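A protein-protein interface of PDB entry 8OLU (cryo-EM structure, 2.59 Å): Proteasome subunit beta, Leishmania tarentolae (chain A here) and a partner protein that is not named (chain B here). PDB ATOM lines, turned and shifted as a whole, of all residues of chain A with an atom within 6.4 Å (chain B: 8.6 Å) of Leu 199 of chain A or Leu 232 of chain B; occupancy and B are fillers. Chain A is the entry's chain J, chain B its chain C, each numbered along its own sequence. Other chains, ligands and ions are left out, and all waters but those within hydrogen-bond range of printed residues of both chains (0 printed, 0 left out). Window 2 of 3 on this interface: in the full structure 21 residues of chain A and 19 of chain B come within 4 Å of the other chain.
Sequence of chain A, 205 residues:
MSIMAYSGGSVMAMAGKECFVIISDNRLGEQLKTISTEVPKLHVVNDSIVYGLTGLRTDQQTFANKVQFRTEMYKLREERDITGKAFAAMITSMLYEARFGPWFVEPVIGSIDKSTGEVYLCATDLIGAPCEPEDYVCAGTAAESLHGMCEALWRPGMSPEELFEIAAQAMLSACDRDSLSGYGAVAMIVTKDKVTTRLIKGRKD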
ATOM      1  N   ASN A  26       8.258 -15.122  16.242  1.00  0.00           N
ATOM      2  CA  ASN A  26       8.387 -16.559  16.446  1.00  0.00           C
ATOM      3  C   ASN A  26       9.366 -17.204  15.472  1.00  0.00           C
ATOM      4  O   ASN A  26       9.531 -18.392  15.456  1.00  0.00           O
ATOM      5  CB  ASN A  26       7.088 -17.276  16.151  1.00  0.00           C
ATOM      6  CG  ASN A  26       6.132 -17.264  17.298  1.00  0.00           C
ATOM      7  OD1 ASN A  26       6.570 -17.531  18.404  1.00  0.00           O
ATOM      8  ND2 ASN A  26       4.853 -16.981  17.028  1.00  0.00           N
ATOM      9  N   PRO A  40       9.702 -18.665  19.949  1.00  0.00           N
ATOM     10  CA  PRO A  40       9.585 -17.441  20.709  1.00  0.00           C
ATOM     11  C   PRO A  40      10.897 -17.235  21.444  1.00  0.00           C
ATOM     12  O   PRO A  40      11.554 -18.196  21.796  1.00  0.00           O
ATOM     13  CB  PRO A  40       8.349 -17.722  21.567  1.00  0.00           C
ATOM     14  CG  PRO A  40       8.371 -19.198  21.701  1.00  0.00           C
ATOM     15  CD  PRO A  40       8.706 -19.662  20.323  1.00  0.00           C
ATOM     16  N   TYR A 183       5.908 -14.826  11.769  1.00  0.00           N
ATOM     17  CA  TYR A 183       5.145 -15.971  12.149  1.00  0.00           C
ATOM     18  C   TYR A 183       4.464 -15.704  13.461  1.00  0.00           C
ATOM     19  O   TYR A 183       4.432 -16.514  14.364  1.00  0.00           O
ATOM     20  CB  TYR A 183       6.032 -17.189  11.998  1.00  0.00           C
ATOM     21  CG  TYR A 183       6.619 -17.337  10.609  1.00  0.00           C
ATOM     22  CD1 TYR A 183       5.937 -17.962   9.599  1.00  0.00           C
ATOM     23  CD2 TYR A 183       7.857 -16.814  10.291  1.00  0.00           C
ATOM     24  CE1 TYR A 183       6.479 -18.082   8.325  1.00  0.00           C
ATOM     25  CE2 TYR A 183       8.398 -16.886   9.009  1.00  0.00           C
ATOM     26  CZ  TYR A 183       7.713 -17.546   8.014  1.00  0.00           C
ATOM     27  OH  TYR A 183       8.254 -17.655   6.766  1.00  0.00           O
ATOM     28  N   GLY A 184       3.764 -14.590  13.505  1.00  0.00           N
ATOM     29  CA  GLY A 184       3.031 -14.244  14.711  1.00  0.00           C
ATOM     30  C   GLY A 184       3.959 -14.088  15.909  1.00  0.00           C
ATOM     31  O   GLY A 184       5.156 -13.942  15.783  1.00  0.00           O
ATOM     32  N   ALA A 185       3.397 -14.101  17.090  1.00  0.00           N
ATOM     33  CA  ALA A 185       4.151 -13.647  18.212  1.00  0.00           C
ATOM     34  C   ALA A 185       3.644 -14.318  19.451  1.00  0.00           C
ATOM     35  O   ALA A 185       2.623 -14.905  19.445  1.00  0.00           O
ATOM     36  CB  ALA A 185       3.998 -12.175  18.235  1.00  0.00           C
ATOM     37  N   VAL A 186       4.469 -14.336  20.470  1.00  0.00           N
ATOM     38  CA  VAL A 186       4.066 -14.753  21.790  1.00  0.00           C
ATOM     39  C   VAL A 186       4.192 -13.577  22.701  1.00  0.00           C
ATOM     40  O   VAL A 186       5.109 -12.819  22.521  1.00  0.00           O
ATOM     41  CB  VAL A 186       4.977 -15.847  22.310  1.00  0.00           C
ATOM     42  CG1 VAL A 186       4.417 -16.387  23.606  1.00  0.00           C
ATOM     43  CG2 VAL A 186       5.014 -16.948  21.292  1.00  0.00           C
ATOM     44  N   ALA A 187       3.293 -13.448  23.652  1.00  0.00           N
ATOM     45  CA  ALA A 187       3.297 -12.242  24.443  1.00  0.00           C
ATOM     46  C   ALA A 187       3.067 -12.643  25.862  1.00  0.00           C
ATOM     47  O   ALA A 187       2.349 -13.579  26.065  1.00  0.00           O
ATOM     48  CB  ALA A 187       2.279 -11.267  23.947  1.00  0.00           C
ATOM     49  N   THR A 197       0.082 -15.629  29.196  1.00  0.00           N
ATOM     50  CA  THR A 197       0.826 -15.789  27.964  1.00  0.00           C
ATOM     51  C   THR A 197      -0.174 -15.907  26.836  1.00  0.00           C
ATOM     52  O   THR A 197      -1.223 -16.478  26.973  1.00  0.00           O
ATOM     53  CB  THR A 197       1.770 -16.991  28.057  1.00  0.00           C
ATOM     54  OG1 THR A 197       2.614 -16.982  29.221  1.00  0.00           O
ATOM     55  CG2 THR A 197       2.708 -17.002  26.868  1.00  0.00           C
ATOM     56  N   ARG A 198       0.122 -15.346  25.701  1.00  0.00           N
ATOM     57  CA  ARG A 198      -0.795 -15.490  24.605  1.00  0.00           C
ATOM     58  C   ARG A 198      -0.028 -15.660  23.332  1.00  0.00           C
ATOM     59  O   ARG A 198       0.920 -14.937  23.093  1.00  0.00           O
ATOM     60  CB  ARG A 198      -1.643 -14.242  24.475  1.00  0.00           C
ATOM     61  CG  ARG A 198      -2.562 -14.065  25.668  1.00  0.00           C
ATOM     62  CD  ARG A 198      -3.548 -13.000  25.307  1.00  0.00           C
ATOM     63  NE  ARG A 198      -4.418 -12.632  26.408  1.00  0.00           N
ATOM     64  CZ  ARG A 198      -5.119 -11.512  26.399  1.00  0.00           C
ATOM     65  NH1 ARG A 198      -5.028 -10.708  25.349  1.00  0.00           N
ATOM     66  NH2 ARG A 198      -5.838 -11.178  27.453  1.00  0.00           N
ATOM     67  N   LEU A 199      -0.478 -16.607  22.532  1.00  0.00           N
ATOM     68  CA  LEU A 199       0.102 -16.825  21.228  1.00  0.00           C
ATOM     69  C   LEU A 199      -0.793 -16.132  20.211  1.00  0.00           C
ATOM     70  O   LEU A 199      -1.964 -16.363  20.153  1.00  0.00           O
ATOM     71  CB  LEU A 199       0.191 -18.339  21.014  1.00  0.00           C
ATOM     72  CG  LEU A 199       0.600 -18.756  19.607  1.00  0.00           C
ATOM     73  CD1 LEU A 199       2.053 -18.415  19.276  1.00  0.00           C
ATOM     74  CD2 LEU A 199       0.393 -20.233  19.418  1.00  0.00           C
ATOM     75  N   ILE A 200      -0.229 -15.258  19.431  1.00  0.00           N
ATOM     76  CA  ILE A 200      -0.946 -14.351  18.588  1.00  0.00           C
ATOM     77  C   ILE A 200      -0.729 -14.803  17.167  1.00  0.00           C
ATOM     78  O   ILE A 200       0.389 -15.135  16.783  1.00  0.00           O
ATOM     79  CB  ILE A 200      -0.321 -12.967  18.792  1.00  0.00           C
ATOM     80  CG1 ILE A 200      -0.562 -12.474  20.199  1.00  0.00           C
ATOM     81  CG2 ILE A 200      -0.760 -11.905  17.781  1.00  0.00           C
ATOM     82  CD1 ILE A 200       0.370 -11.326  20.501  1.00  0.00           C
ATOM     83  N   LYS A 201      -1.803 -14.747  16.389  1.00  0.00           N
ATOM     84  CA  LYS A 201      -1.809 -15.195  15.007  1.00  0.00           C
ATOM     85  C   LYS A 201      -1.200 -14.100  14.167  1.00  0.00           C
ATOM     86  O   LYS A 201      -1.487 -12.928  14.391  1.00  0.00           O
ATOM     87  CB  LYS A 201      -3.265 -15.446  14.646  1.00  0.00           C
ATOM     88  CG  LYS A 201      -3.629 -15.707  13.203  1.00  0.00           C
ATOM     89  CD  LYS A 201      -5.077 -16.222  13.127  1.00  0.00           C
ATOM     90  CE  LYS A 201      -5.926 -15.475  12.113  1.00  0.00           C
ATOM     91  NZ  LYS A 201      -5.293 -15.475  10.766  1.00  0.00           N
ATOM     92  N   ILE B 229       4.560 -24.657  34.107  1.00  0.00           N
ATOM     93  CA  ILE B 229       4.578 -25.058  32.709  1.00  0.00           C
ATOM     94  C   ILE B 229       4.265 -23.815  31.857  1.00  0.00           C
ATOM     95  O   ILE B 229       3.097 -23.468  31.668  1.00  0.00           O
ATOM     96  CB  ILE B 229       3.605 -26.247  32.470  1.00  0.00           C
ATOM     97  CG1 ILE B 229       3.272 -26.442  30.978  1.00  0.00           C
ATOM     98  CG2 ILE B 229       2.341 -26.128  33.327  1.00  0.00           C
ATOM     99  CD1 ILE B 229       2.430 -27.674  30.635  1.00  0.00           C
ATOM    100  N   ASP B 230       5.313 -23.116  31.377  1.00  0.00           N
ATOM    101  CA  ASP B 230       5.155 -22.080  30.357  1.00  0.00           C
ATOM    102  C   ASP B 230       5.362 -22.710  28.973  1.00  0.00           C
ATOM    103  O   ASP B 230       6.478 -22.752  28.461  1.00  0.00           O
ATOM    104  CB  ASP B 230       6.115 -20.900  30.568  1.00  0.00           C
ATOM    105  CG  ASP B 230       5.748 -19.927  31.684  1.00  0.00           C
ATOM    106  OD1 ASP B 230       4.709 -19.236  31.555  1.00  0.00           O
ATOM    107  OD2 ASP B 230       6.526 -19.843  32.668  1.00  0.00           O
ATOM    108  N   GLN B 231       4.274 -23.213  28.374  1.00  0.00           N
ATOM    109  CA  GLN B 231       4.382 -24.064  27.202  1.00  0.00           C
ATOM    110  C   GLN B 231       4.328 -23.256  25.901  1.00  0.00           C
ATOM    111  O   GLN B 231       4.788 -23.710  24.866  1.00  0.00           O
ATOM    112  CB  GLN B 231       3.280 -25.128  27.183  1.00  0.00           C
ATOM    113  CG  GLN B 231       3.494 -26.232  26.139  1.00  0.00           C
ATOM    114  CD  GLN B 231       4.610 -27.199  26.485  1.00  0.00           C
ATOM    115  OE1 GLN B 231       4.447 -28.096  27.311  1.00  0.00           O
ATOM    116  NE2 GLN B 231       5.764 -27.008  25.874  1.00  0.00           N
ATOM    117  N   LEU B 232       3.764 -22.060  25.896  1.00  0.00           N
ATOM    118  CA  LEU B 232       3.843 -21.298  24.672  1.00  0.00           C
ATOM    119  C   LEU B 232       5.260 -20.809  24.457  1.00  0.00           C
ATOM    120  O   LEU B 232       5.636 -20.547  23.326  1.00  0.00           O
ATOM    121  CB  LEU B 232       2.843 -20.149  24.720  1.00  0.00           C
ATOM    122  CG  LEU B 232       1.390 -20.593  24.864  1.00  0.00           C
ATOM    123  CD1 LEU B 232       0.448 -19.407  24.676  1.00  0.00           C
ATOM    124  CD2 LEU B 232       1.070 -21.722  23.890  1.00  0.00           C
ATOM    125  N   LEU B 233       6.041 -20.749  25.533  1.00  0.00           N
ATOM    126  CA  LEU B 233       7.367 -20.165  25.487  1.00  0.00           C
ATOM    127  C   LEU B 233       8.452 -21.091  24.938  1.00  0.00           C
ATOM    128  O   LEU B 233       9.434 -20.578  24.407  1.00  0.00           O
ATOM    129  CB  LEU B 233       7.747 -19.708  26.891  1.00  0.00           C
ATOM    130  CG  LEU B 233       7.196 -18.348  27.334  1.00  0.00           C
ATOM    131  CD1 LEU B 233       8.221 -17.682  28.237  1.00  0.00           C
ATOM    132  CD2 LEU B 233       6.816 -17.397  26.204  1.00  0.00           C
ATOM    133  N   ASP B 234       8.369 -22.410  25.142  1.00  0.00           N
ATOM    134  CA  ASP B 234       9.083 -23.360  24.293  1.00  0.00           C
ATOM    135  C   ASP B 234       8.109 -24.491  24.013  1.00  0.00           C
ATOM    136  O   ASP B 234       7.768 -25.264  24.901  1.00  0.00           O
ATOM    137  CB  ASP B 234      10.441 -23.842  24.852  1.00  0.00           C
ATOM    138  CG  ASP B 234      11.338 -24.658  23.881  1.00  0.00           C
ATOM    139  OD1 ASP B 234      10.868 -25.042  22.746  1.00  0.00           O
ATOM    140  OD2 ASP B 234      12.534 -24.943  24.256  1.00  0.00           O
ATOM    141  N   PRO B 235       7.563 -24.521  22.792  1.00  0.00           N
ATOM    142  CA  PRO B 235       6.540 -25.481  22.407  1.00  0.00           C
ATOM    143  C   PRO B 235       6.913 -26.943  22.350  1.00  0.00           C
ATOM    144  O   PRO B 235       6.057 -27.802  22.490  1.00  0.00           O
ATOM    145  CB  PRO B 235       6.273 -25.098  20.956  1.00  0.00           C
ATOM    146  CG  PRO B 235       6.545 -23.602  20.928  1.00  0.00           C
ATOM    147  CD  PRO B 235       7.792 -23.495  21.768  1.00  0.00           C
ATOM    148  N   PHE B 236       8.186 -27.198  22.080  1.00  0.00           N
ATOM    149  CA  PHE B 236       8.667 -28.548  21.883  1.00  0.00           C
ATOM    150  C   PHE B 236       9.148 -29.116  23.200  1.00  0.00           C
ATOM    151  O   PHE B 236       9.282 -30.315  23.313  1.00  0.00           O
ATOM    152  CB  PHE B 236       9.774 -28.553  20.841  1.00  0.00           C
ATOM    153  CG  PHE B 236       9.280 -28.127  19.483  1.00  0.00           C
ATOM    154  CD1 PHE B 236       8.624 -29.029  18.661  1.00  0.00           C
ATOM    155  CD2 PHE B 236       9.433 -26.814  19.052  1.00  0.00           C
ATOM    156  CE1 PHE B 236       8.159 -28.636  17.416  1.00  0.00           C
ATOM    157  CE2 PHE B 236       8.962 -26.424  17.811  1.00  0.00           C
ATOM    158  CZ  PHE B 236       8.321 -27.335  17.002  1.00  0.00           C
ATOM    159  N   LYS B 237       9.363 -28.272  24.194  1.00  0.00           N
ATOM    160  CA  LYS B 237       9.923 -28.751  25.437  1.00  0.00           C
ATOM    161  C   LYS B 237       8.839 -29.516  26.191  1.00  0.00           C
ATOM    162  O   LYS B 237       7.690 -29.092  26.242  1.00  0.00           O
ATOM    163  CB  LYS B 237      10.467 -27.574  26.247  1.00  0.00           C
ATOM    164  CG  LYS B 237      11.642 -27.895  27.166  1.00  0.00           C
ATOM    165  CD  LYS B 237      12.212 -26.651  27.854  1.00  0.00           C
ATOM    166  CE  LYS B 237      13.171 -26.982  28.978  1.00  0.00           C
ATOM    167  NZ  LYS B 237      12.520 -27.824  30.012  1.00  0.00           N
ATOM    168  N   HIS B 239       7.409 -30.833  29.711  1.00  0.00           N
ATOM    169  CA  HIS B 239       7.413 -30.448  31.100  1.00  0.00           C
ATOM    170  C   HIS B 239       6.707 -31.552  31.852  1.00  0.00           C
ATOM    171  O   HIS B 239       5.575 -31.887  31.517  1.00  0.00           O
ATOM    172  CB  HIS B 239       6.685 -29.112  31.268  1.00  0.00           C
ATOM    173  CG  HIS B 239       7.437 -27.932  30.739  1.00  0.00           C
ATOM    174  ND1 HIS B 239       7.005 -27.175  29.669  1.00  0.00           N
ATOM    175  CD2 HIS B 239       8.640 -27.430  31.161  1.00  0.00           C
ATOM    176  CE1 HIS B 239       7.902 -26.216  29.435  1.00  0.00           C
ATOM    177  NE2 HIS B 239       8.932 -26.360  30.355  1.00  0.00           N
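Of the printed residues of chain B, Leu 199 of chain A touches Leu 232 (3.6 Å). Printed residues of chain A within 4 Å of Leu 232 of chain B: Pro 40, Thr 197 and Leu 199. Of the printed residues of chain B, Thr 197 of chain A touches Asp 230 and Leu 232. Of the printed residues of chain B, Val 186 of chain A touches Leu 233 (3.7 Å). Pro 235 of chain B touches none of the printed residues of chain A.
Pro 40 of chain A touches Leu 232 of chain B (CG to O, 3.5 Å). Pro 40 of chain A touches Leu 233 of chain B (CG to O, 3.2 Å). Val 186 of chain A touches Leu 233 of chain B (CG1 to CD2, 3.7 Å). Asp 230 of chain B touches Thr 197 of chain A (OD1 to OG1, 3.9 Å). Thr 197 of chain A touches Leu 232 of chain B. Leu 199 of chain A touches Leu 232 of chain B.
Of the 10 printed residues of chain B, 3 touch a printed residue of chain A. Among the printed residues, 6 pairs touch across the chains. Among the printed residues, no Asp or Glu carboxylate lies within 4 Å of a Lys or Arg side-chain nitrogen of the other chain.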
